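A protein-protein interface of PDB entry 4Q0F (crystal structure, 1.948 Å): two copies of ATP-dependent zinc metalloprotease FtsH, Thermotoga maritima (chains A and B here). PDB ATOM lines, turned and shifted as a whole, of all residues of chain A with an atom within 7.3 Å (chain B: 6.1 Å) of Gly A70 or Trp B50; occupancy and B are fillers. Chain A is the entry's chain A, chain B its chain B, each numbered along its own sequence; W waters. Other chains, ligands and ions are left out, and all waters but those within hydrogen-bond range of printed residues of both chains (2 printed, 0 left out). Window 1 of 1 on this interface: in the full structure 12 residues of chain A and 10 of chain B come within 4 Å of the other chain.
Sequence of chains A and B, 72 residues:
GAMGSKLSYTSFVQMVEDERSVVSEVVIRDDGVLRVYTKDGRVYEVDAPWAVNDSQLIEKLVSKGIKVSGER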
ATOM      1  N   VAL A  26       3.997  19.627  13.524  1.00  0.00           N
ATOM      2  CA  VAL A  26       2.872  19.875  12.636  1.00  0.00           C
ATOM      3  C   VAL A  26       3.384  20.047  11.212  1.00  0.00           C
ATOM      4  O   VAL A  26       4.170  20.952  10.931  1.00  0.00           O
ATOM      5  CB  VAL A  26       2.083  21.136  13.041  1.00  0.00           C
ATOM      6  CG1 VAL A  26       0.972  21.409  12.039  1.00  0.00           C
ATOM      7  CG2 VAL A  26       1.513  20.985  14.445  1.00  0.00           C
ATOM      8  N   VAL A  27       2.950  19.165  10.320  1.00  0.00           N
ATOM      9  CA  VAL A  27       3.318  19.266   8.915  1.00  0.00           C
ATOM     10  C   VAL A  27       2.183  19.913   8.135  1.00  0.00           C
ATOM     11  O   VAL A  27       1.052  19.431   8.152  1.00  0.00           O
ATOM     12  CB  VAL A  27       3.639  17.890   8.308  1.00  0.00           C
ATOM     13  CG1 VAL A  27       3.975  18.031   6.833  1.00  0.00           C
ATOM     14  CG2 VAL A  27       4.789  17.235   9.058  1.00  0.00           C
ATOM     15  N   ILE A  28       2.490  21.012   7.458  1.00  0.00           N
ATOM     16  CA  ILE A  28       1.481  21.757   6.720  1.00  0.00           C
ATOM     17  C   ILE A  28       1.571  21.465   5.225  1.00  0.00           C
ATOM     18  O   ILE A  28       2.442  21.988   4.530  1.00  0.00           O
ATOM     19  CB  ILE A  28       1.615  23.271   6.971  1.00  0.00           C
ATOM     20  CG1 ILE A  28       1.553  23.565   8.473  1.00  0.00           C
ATOM     21  CG2 ILE A  28       0.528  24.034   6.241  1.00  0.00           C
ATOM     22  CD1 ILE A  28       1.712  25.029   8.818  1.00  0.00           C
ATOM     23  N   ARG A  29       0.671  20.616   4.739  1.00  0.00           N
ATOM     24  CA  ARG A  29       0.655  20.234   3.332  1.00  0.00           C
ATOM     25  C   ARG A  29      -0.004  21.313   2.483  1.00  0.00           C
ATOM     26  O   ARG A  29      -0.883  22.034   2.953  1.00  0.00           O
ATOM     27  CB  ARG A  29      -0.083  18.910   3.145  1.00  0.00           C
ATOM     28  CG  ARG A  29       0.562  17.723   3.835  1.00  0.00           C
ATOM     29  CD  ARG A  29      -0.336  16.498   3.752  1.00  0.00           C
ATOM     30  NE  ARG A  29      -0.961  16.370   2.438  1.00  0.00           N
ATOM     31  CZ  ARG A  29      -0.377  15.812   1.382  1.00  0.00           C
ATOM     32  NH1 ARG A  29       0.854  15.330   1.480  1.00  0.00           N
ATOM     33  NH2 ARG A  29      -1.023  15.739   0.227  1.00  0.00           N
ATOM     34  N   ASP A  30       0.410  21.410   1.224  1.00  0.00           N
ATOM     35  CA  ASP A  30      -0.097  22.452   0.336  1.00  0.00           C
ATOM     36  C   ASP A  30      -1.527  22.188  -0.138  1.00  0.00           C
ATOM     37  O   ASP A  30      -2.152  23.055  -0.748  1.00  0.00           O
ATOM     38  CB  ASP A  30       0.842  22.652  -0.858  1.00  0.00           C
ATOM     39  CG  ASP A  30       0.998  21.400  -1.698  1.00  0.00           C
ATOM     40  OD1 ASP A  30       0.567  20.317  -1.251  1.00  0.00           O
ATOM     41  OD2 ASP A  30       1.565  21.499  -2.808  1.00  0.00           O
ATOM     42  N   ALA A  51      -5.893  26.853   7.699  1.00  0.00           N
ATOM     43  CA  ALA A  51      -4.712  26.936   8.553  1.00  0.00           C
ATOM     44  C   ALA A  51      -3.455  27.154   7.718  1.00  0.00           C
ATOM     45  O   ALA A  51      -2.473  27.722   8.195  1.00  0.00           O
ATOM     46  CB  ALA A  51      -4.580  25.675   9.391  1.00  0.00           C
ATOM     47  N   VAL A  52      -3.512  26.700   6.469  1.00  0.00           N
ATOM     48  CA  VAL A  52      -2.381  26.738   5.539  1.00  0.00           C
ATOM     49  C   VAL A  52      -1.746  28.118   5.389  1.00  0.00           C
ATOM     50  O   VAL A  52      -0.522  28.247   5.353  1.00  0.00           O
ATOM     51  CB  VAL A  52      -2.777  26.152   4.157  1.00  0.00           C
ATOM     52  CG1 VAL A  52      -2.522  27.136   3.023  1.00  0.00           C
ATOM     53  CG2 VAL A  52      -2.037  24.856   3.914  1.00  0.00           C
ATOM     54  N   ASN A  53      -2.572  29.152   5.301  1.00  0.00           N
ATOM     55  CA  ASN A  53      -2.060  30.512   5.368  1.00  0.00           C
ATOM     56  C   ASN A  53      -2.626  31.210   6.610  1.00  0.00           C
ATOM     57  O   ASN A  53      -3.459  32.094   6.492  1.00  0.00           O
ATOM     58  CB  ASN A  53      -2.356  31.294   4.066  1.00  0.00           C
ATOM     59  CG  ASN A  53      -3.824  31.235   3.654  1.00  0.00           C
ATOM     60  OD1 ASN A  53      -4.664  30.702   4.382  1.00  0.00           O
ATOM     61  ND2 ASN A  53      -4.138  31.792   2.486  1.00  0.00           N
ATOM     62  N   ASP A  54      -2.190  30.785   7.797  1.00  0.00           N
ATOM     63  CA  ASP A  54      -2.697  31.326   9.059  1.00  0.00           C
ATOM     64  C   ASP A  54      -1.493  31.730   9.888  1.00  0.00           C
ATOM     65  O   ASP A  54      -1.056  30.998  10.777  1.00  0.00           O
ATOM     66  CB  ASP A  54      -3.521  30.286   9.795  1.00  0.00           C
ATOM     67  CG  ASP A  54      -4.700  30.874  10.534  1.00  0.00           C
ATOM     68  OD1 ASP A  54      -5.024  32.077  10.371  1.00  0.00           O
ATOM     69  OD2 ASP A  54      -5.339  30.099  11.303  1.00  0.00           O
ATOM     70  N   SER A  55      -0.959  32.906   9.576  1.00  0.00           N
ATOM     71  CA  SER A  55       0.270  33.406  10.183  1.00  0.00           C
ATOM     72  C   SER A  55       0.303  33.376  11.722  1.00  0.00           C
ATOM     73  O   SER A  55       1.313  32.989  12.306  1.00  0.00           O
ATOM     74  CB  SER A  55       0.537  34.812   9.663  1.00  0.00           C
ATOM     75  OG  SER A  55       1.740  35.304  10.190  1.00  0.00           O
ATOM     76  N   ILE A  58       0.613  29.791  12.957  1.00  0.00           N
ATOM     77  CA  ILE A  58       1.966  29.315  12.710  1.00  0.00           C
ATOM     78  C   ILE A  58       2.949  29.893  13.722  1.00  0.00           C
ATOM     79  O   ILE A  58       3.754  29.165  14.297  1.00  0.00           O
ATOM     80  CB  ILE A  58       2.412  29.650  11.278  1.00  0.00           C
ATOM     81  CG1 ILE A  58       1.506  28.929  10.278  1.00  0.00           C
ATOM     82  CG2 ILE A  58       3.867  29.272  11.063  1.00  0.00           C
ATOM     83  CD1 ILE A  58       1.711  29.352   8.850  1.00  0.00           C
ATOM     84  N   GLU A  59       2.871  31.196  13.963  1.00  0.00           N
ATOM     85  CA  GLU A  59       3.767  31.811  14.936  1.00  0.00           C
ATOM     86  C   GLU A  59       3.454  31.376  16.370  1.00  0.00           C
ATOM     87  O   GLU A  59       4.344  31.357  17.222  1.00  0.00           O
ATOM     88  CB  GLU A  59       3.781  33.334  14.796  1.00  0.00           C
ATOM     89  CG  GLU A  59       4.365  33.815  13.472  1.00  0.00           C
ATOM     90  CD  GLU A  59       5.759  33.268  13.205  1.00  0.00           C
ATOM     91  OE1 GLU A  59       6.610  33.316  14.120  1.00  0.00           O
ATOM     92  OE2 GLU A  59       6.003  32.787  12.078  1.00  0.00           O
ATOM     93  N   VAL A  62       5.203  27.987  16.508  1.00  0.00           N
ATOM     94  CA  VAL A  62       6.645  28.202  16.581  1.00  0.00           C
ATOM     95  C   VAL A  62       7.073  28.692  17.961  1.00  0.00           C
ATOM     96  O   VAL A  62       8.051  28.196  18.524  1.00  0.00           O
ATOM     97  CB  VAL A  62       7.124  29.200  15.506  1.00  0.00           C
ATOM     98  CG1 VAL A  62       8.575  29.593  15.746  1.00  0.00           C
ATOM     99  CG2 VAL A  62       6.951  28.606  14.116  1.00  0.00           C
ATOM    100  N   VAL A  68       7.362  23.045  13.010  1.00  0.00           N
ATOM    101  CA  VAL A  68       6.447  23.339  11.916  1.00  0.00           C
ATOM    102  C   VAL A  68       7.178  23.266  10.586  1.00  0.00           C
ATOM    103  O   VAL A  68       8.219  23.896  10.406  1.00  0.00           O
ATOM    104  CB  VAL A  68       5.830  24.742  12.058  1.00  0.00           C
ATOM    105  CG1 VAL A  68       4.899  25.037  10.892  1.00  0.00           C
ATOM    106  CG2 VAL A  68       5.090  24.863  13.375  1.00  0.00           C
ATOM    107  N   SER A  69       6.633  22.493   9.654  1.00  0.00           N
ATOM    108  CA  SER A  69       7.231  22.395   8.329  1.00  0.00           C
ATOM    109  C   SER A  69       6.197  22.251   7.222  1.00  0.00           C
ATOM    110  O   SER A  69       5.124  21.683   7.425  1.00  0.00           O
ATOM    111  CB  SER A  69       8.240  21.247   8.270  1.00  0.00           C
ATOM    112  OG  SER A  69       7.704  20.060   8.824  1.00  0.00           O
ATOM    113  N   GLY A  70       6.528  22.782   6.049  1.00  0.00           N
ATOM    114  CA  GLY A  70       5.666  22.666   4.891  1.00  0.00           C
ATOM    115  C   GLY A  70       5.969  21.398   4.120  1.00  0.00           C
ATOM    116  O   GLY A  70       7.058  20.832   4.236  1.00  0.00           O
ATOM    117  N   GLU A  71       5.000  20.949   3.332  1.00  0.00           N
ATOM    118  CA  GLU A  71       5.156  19.734   2.548  1.00  0.00           C
ATOM    119  C   GLU A  71       4.430  19.880   1.218  1.00  0.00           C
ATOM    120  O   GLU A  71       3.372  20.504   1.146  1.00  0.00           O
ATOM    121  CB  GLU A  71       4.610  18.533   3.326  1.00  0.00           C
ATOM    122  CG  GLU A  71       4.880  17.185   2.682  1.00  0.00           C
ATOM    123  CD  GLU A  71       4.382  16.028   3.531  1.00  0.00           C
ATOM    124  OE1 GLU A  71       3.241  15.569   3.306  1.00  0.00           O
ATOM    125  OE2 GLU A  71       5.131  15.579   4.424  1.00  0.00           O
ATOM    126  N   ARG A  72       5.007  19.311   0.164  1.00  0.00           N
ATOM    127  CA  ARG A  72       4.392  19.356  -1.157  1.00  0.00           C
ATOM    128  C   ARG A  72       4.703  18.088  -1.947  1.00  0.00           C
ATOM    129  O   ARG A  72       4.070  17.810  -2.966  1.00  0.00           O
ATOM    130  CB  ARG A  72       4.863  20.588  -1.928  1.00  0.00           C
ATOM    131  CG  ARG A  72       6.326  20.547  -2.338  1.00  0.00           C
ATOM    132  CD  ARG A  72       6.758  21.874  -2.939  1.00  0.00           C
ATOM    133  NE  ARG A  72       6.715  22.948  -1.952  1.00  0.00           N
ATOM    134  CZ  ARG A  72       6.745  24.243  -2.252  1.00  0.00           C
ATOM    135  NH1 ARG A  72       6.806  24.633  -3.518  1.00  0.00           N
ATOM    136  NH2 ARG A  72       6.704  25.148  -1.284  1.00  0.00           N
ATOM    137  N   TYR B   9      10.536  25.137   9.434  1.00  0.00           N
ATOM    138  CA  TYR B   9      10.292  26.567   9.577  1.00  0.00           C
ATOM    139  C   TYR B   9      10.597  27.023  10.998  1.00  0.00           C
ATOM    140  O   TYR B   9      11.126  28.116  11.212  1.00  0.00           O
ATOM    141  CB  TYR B   9       8.849  26.915   9.212  1.00  0.00           C
ATOM    142  CG  TYR B   9       8.541  28.388   9.350  1.00  0.00           C
ATOM    143  CD1 TYR B   9       9.087  29.315   8.470  1.00  0.00           C
ATOM    144  CD2 TYR B   9       7.711  28.854  10.361  1.00  0.00           C
ATOM    145  CE1 TYR B   9       8.814  30.663   8.595  1.00  0.00           C
ATOM    146  CE2 TYR B   9       7.432  30.203  10.491  1.00  0.00           C
ATOM    147  CZ  TYR B   9       7.987  31.101   9.605  1.00  0.00           C
ATOM    148  OH  TYR B   9       7.714  32.442   9.727  1.00  0.00           O
ATOM    149  N   GLY B  32       7.562  29.239  -2.733  1.00  0.00           N
ATOM    150  CA  GLY B  32       7.365  29.055  -1.307  1.00  0.00           C
ATOM    151  C   GLY B  32       8.515  28.358  -0.606  1.00  0.00           C
ATOM    152  O   GLY B  32       8.386  27.949   0.548  1.00  0.00           O
ATOM    153  N   ASP B  47      10.571  24.672   3.351  1.00  0.00           N
ATOM    154  CA  ASP B  47       9.270  24.707   2.693  1.00  0.00           C
ATOM    155  C   ASP B  47       8.305  25.527   3.540  1.00  0.00           C
ATOM    156  O   ASP B  47       7.835  25.066   4.580  1.00  0.00           O
ATOM    157  CB  ASP B  47       8.735  23.286   2.492  1.00  0.00           C
ATOM    158  CG  ASP B  47       7.593  23.223   1.492  1.00  0.00           C
ATOM    159  OD1 ASP B  47       6.788  24.175   1.429  1.00  0.00           O
ATOM    160  OD2 ASP B  47       7.502  22.213   0.761  1.00  0.00           O
ATOM    161  N   ALA B  48       8.014  26.746   3.095  1.00  0.00           N
ATOM    162  CA  ALA B  48       7.159  27.648   3.862  1.00  0.00           C
ATOM    163  C   ALA B  48       6.459  28.679   2.982  1.00  0.00           C
ATOM    164  O   ALA B  48       6.867  29.841   2.941  1.00  0.00           O
ATOM    165  CB  ALA B  48       7.970  28.344   4.947  1.00  0.00           C
ATOM    166  N   PRO B  49       5.394  28.257   2.281  1.00  0.00           N
ATOM    167  CA  PRO B  49       4.621  29.126   1.385  1.00  0.00           C
ATOM    168  C   PRO B  49       4.054  30.347   2.102  1.00  0.00           C
ATOM    169  O   PRO B  49       3.854  31.391   1.481  1.00  0.00           O
ATOM    170  CB  PRO B  49       3.474  28.220   0.928  1.00  0.00           C
ATOM    171  CG  PRO B  49       4.002  26.840   1.070  1.00  0.00           C
ATOM    172  CD  PRO B  49       4.881  26.875   2.283  1.00  0.00           C
ATOM    173  N   TRP B  50       3.806  30.211   3.399  1.00  0.00           N
ATOM    174  CA  TRP B  50       3.230  31.289   4.195  1.00  0.00           C
ATOM    175  C   TRP B  50       4.200  32.447   4.416  1.00  0.00           C
ATOM    176  O   TRP B  50       3.805  33.517   4.875  1.00  0.00           O
ATOM    177  CB  TRP B  50       2.760  30.749   5.546  1.00  0.00           C
ATOM    178  CG  TRP B  50       3.823  29.999   6.294  1.00  0.00           C
ATOM    179  CD1 TRP B  50       4.779  30.529   7.112  1.00  0.00           C
ATOM    180  CD2 TRP B  50       4.028  28.579   6.304  1.00  0.00           C
ATOM    181  NE1 TRP B  50       5.570  29.528   7.625  1.00  0.00           N
ATOM    182  CE2 TRP B  50       5.130  28.325   7.146  1.00  0.00           C
ATOM    183  CE3 TRP B  50       3.391  27.504   5.680  1.00  0.00           C
ATOM    184  CZ2 TRP B  50       5.606  27.035   7.378  1.00  0.00           C
ATOM    185  CZ3 TRP B  50       3.866  26.224   5.915  1.00  0.00           C
ATOM    186  CH2 TRP B  50       4.962  26.001   6.756  1.00  0.00           C
ATOM    187  N   ALA B  51       5.468  32.232   4.086  1.00  0.00           N
ATOM    188  CA  ALA B  51       6.497  33.235   4.339  1.00  0.00           C
ATOM    189  C   ALA B  51       6.801  34.105   3.119  1.00  0.00           C
ATOM    190  O   ALA B  51       7.551  35.076   3.221  1.00  0.00           O
ATOM    191  CB  ALA B  51       7.767  32.566   4.840  1.00  0.00           C
ATOM    192  N   VAL B  52       6.214  33.759   1.976  1.00  0.00           N
ATOM    193  CA  VAL B  52       6.539  34.412   0.705  1.00  0.00           C
ATOM    194  C   VAL B  52       6.373  35.934   0.716  1.00  0.00           C
ATOM    195  O   VAL B  52       7.336  36.670   0.500  1.00  0.00           O
ATOM    196  CB  VAL B  52       5.737  33.810  -0.468  1.00  0.00           C
ATOM    197  CG1 VAL B  52       5.960  34.616  -1.737  1.00  0.00           C
ATOM    198  CG2 VAL B  52       6.132  32.361  -0.683  1.00  0.00           C
ATOM    199  N   ASN B  53       5.155  36.407   0.963  1.00  0.00           N
ATOM    200  CA  ASN B  53       4.902  37.843   1.002  1.00  0.00           C
ATOM    201  C   ASN B  53       4.724  38.361   2.426  1.00  0.00           C
ATOM    202  O   ASN B  53       3.929  39.268   2.675  1.00  0.00           O
ATOM    203  CB  ASN B  53       3.690  38.209   0.138  1.00  0.00           C
ATOM    204  CG  ASN B  53       3.970  38.078  -1.348  1.00  0.00           C
ATOM    205  OD1 ASN B  53       3.256  37.380  -2.068  1.00  0.00           O
ATOM    206  ND2 ASN B  53       5.016  38.754  -1.814  1.00  0.00           N
ATOM    207  N   ASP B  54       5.479  37.778   3.354  1.00  0.00           N
ATOM    208  CA  ASP B  54       5.423  38.161   4.760  1.00  0.00           C
ATOM    209  C   ASP B  54       6.306  39.379   5.021  1.00  0.00           C
ATOM    210  O   ASP B  54       7.522  39.256   5.170  1.00  0.00           O
ATOM    211  CB  ASP B  54       5.871  36.991   5.643  1.00  0.00           C
ATOM    212  CG  ASP B  54       5.522  37.190   7.112  1.00  0.00           C
ATOM    213  OD1 ASP B  54       5.406  38.349   7.560  1.00  0.00           O
ATOM    214  OD2 ASP B  54       5.368  36.176   7.825  1.00  0.00           O
HETATM  215  O   HOH W   1       9.081  24.175   6.703  1.00  0.00           O
HETATM  216  O   HOH W   2       4.314  23.597   0.785  1.00  0.00           O
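Ile A28 touches Trp B50 (CD1 to CZ3, 3.8 Å). Trp B50 touches Val A52 (CE3 to O, 3.996 Å). Ile A58 touches Tyr B9. CD1 of Ile A58 touches CG of Trp B50, 3.4 Å away. Val A62 touches Tyr B9. C of Ser A69 touches CH2 of Trp B50, at 3.98 Å. N of Gly A70 touches CH2 of Trp B50, 3.6 Å away. Glu A71 touches Asp B47. O of Gly B32 touches NH2 of Arg A72, 3.7 Å away. Arg A72 touches Pro B49 (NH2 to CG, 3.96 Å).
Water W1 lies within hydrogen-bond range of O of Asp B47 (2.6 Å), N of Gly A70 (3.0 Å) and N of Tyr B9 (3.2 Å). Water W2 bridges OD1 of Asp B47 (2.6 Å) and O of Glu A71 (3.3 Å).
Positions printed for both chains: 51, 52, 53 and 54. Of the 14 pairs that touch across the chains among the printed residues, none has its exchanged pair printed and touching as well.
Of the 10 printed residues of chain B, 5 touch a printed residue of chain A. Hydrophobic or aromatic side chains of chain B within 4 Å of the printed part of chain A: Tyr B9, Pro B49 and Trp B50. Of the 18 printed residues of chain A, 10 touch a printed residue of chain B. Among the printed residues, 14 pairs touch across the chains. Among the printed residues, Asp or Glu carboxylates within 4 Å of a Lys or Arg side-chain nitrogen of the other chain: Arg A72 with Asp B47 (2.9 Å).
The backbone NH (N) of Ser A69 lies within hydrogen-bond range of the backbone carbonyl oxygen (O) of Val A26, at 3.2 Å. The backbone NH (N) of Ile A28 sits at hydrogen-bond distance from the backbone carbonyl oxygen (O) of Ser A69, at 2.7 Å. The backbone carbonyl oxygen (O) of Ile A28 is in hydrogen-bond range of the backbone NH (N) of Glu A71. The guanidinium group (NH1) of Arg A29 lies within salt-bridge range of the side-chain carboxylate (OE1) of Glu A71, at 3.0 Å. The backbone NH of Asp A30 is in hydrogen-bond range of the backbone carbonyl oxygen of Glu A71. The backbone NH (N) of Ala B48 sits at hydrogen-bond distance from the backbone carbonyl oxygen (O) of Gly B32 (2.8 Å).
Gly A70 touches just these residues of chain B: Asp B47 and Trp B50. Printed residues of chain A within 4 Å of Trp B50: Ile A28, Val A52, Ile A58, Ser A69 and Gly A70. Of the printed residues of chain A, Pro B49 touches Arg A72. Printed residues of chain B within 4 Å of Val A62: Tyr B9. Val A27 touches none of the printed residues of chain B. The nearest printed residue of chain B that does not touch Ile A58 is Ala B51 (6.7 Å).
The side-chain carboxylate (OE2) of Glu A59 lies within hydrogen-bond range of the side-chain hydroxyl (OH) of Tyr B9 (2.9 Å). N of Tyr B9 sits at hydrogen-bond distance from O of Val A68 (2.8 Å). O of Asp B47 lies within hydrogen-bond range of N of Gly A70 (3.0 Å). The side-chain carboxylate of Asp B47 is in salt-bridge range of the guanidinium group of Arg A72, 2.9 Å away.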
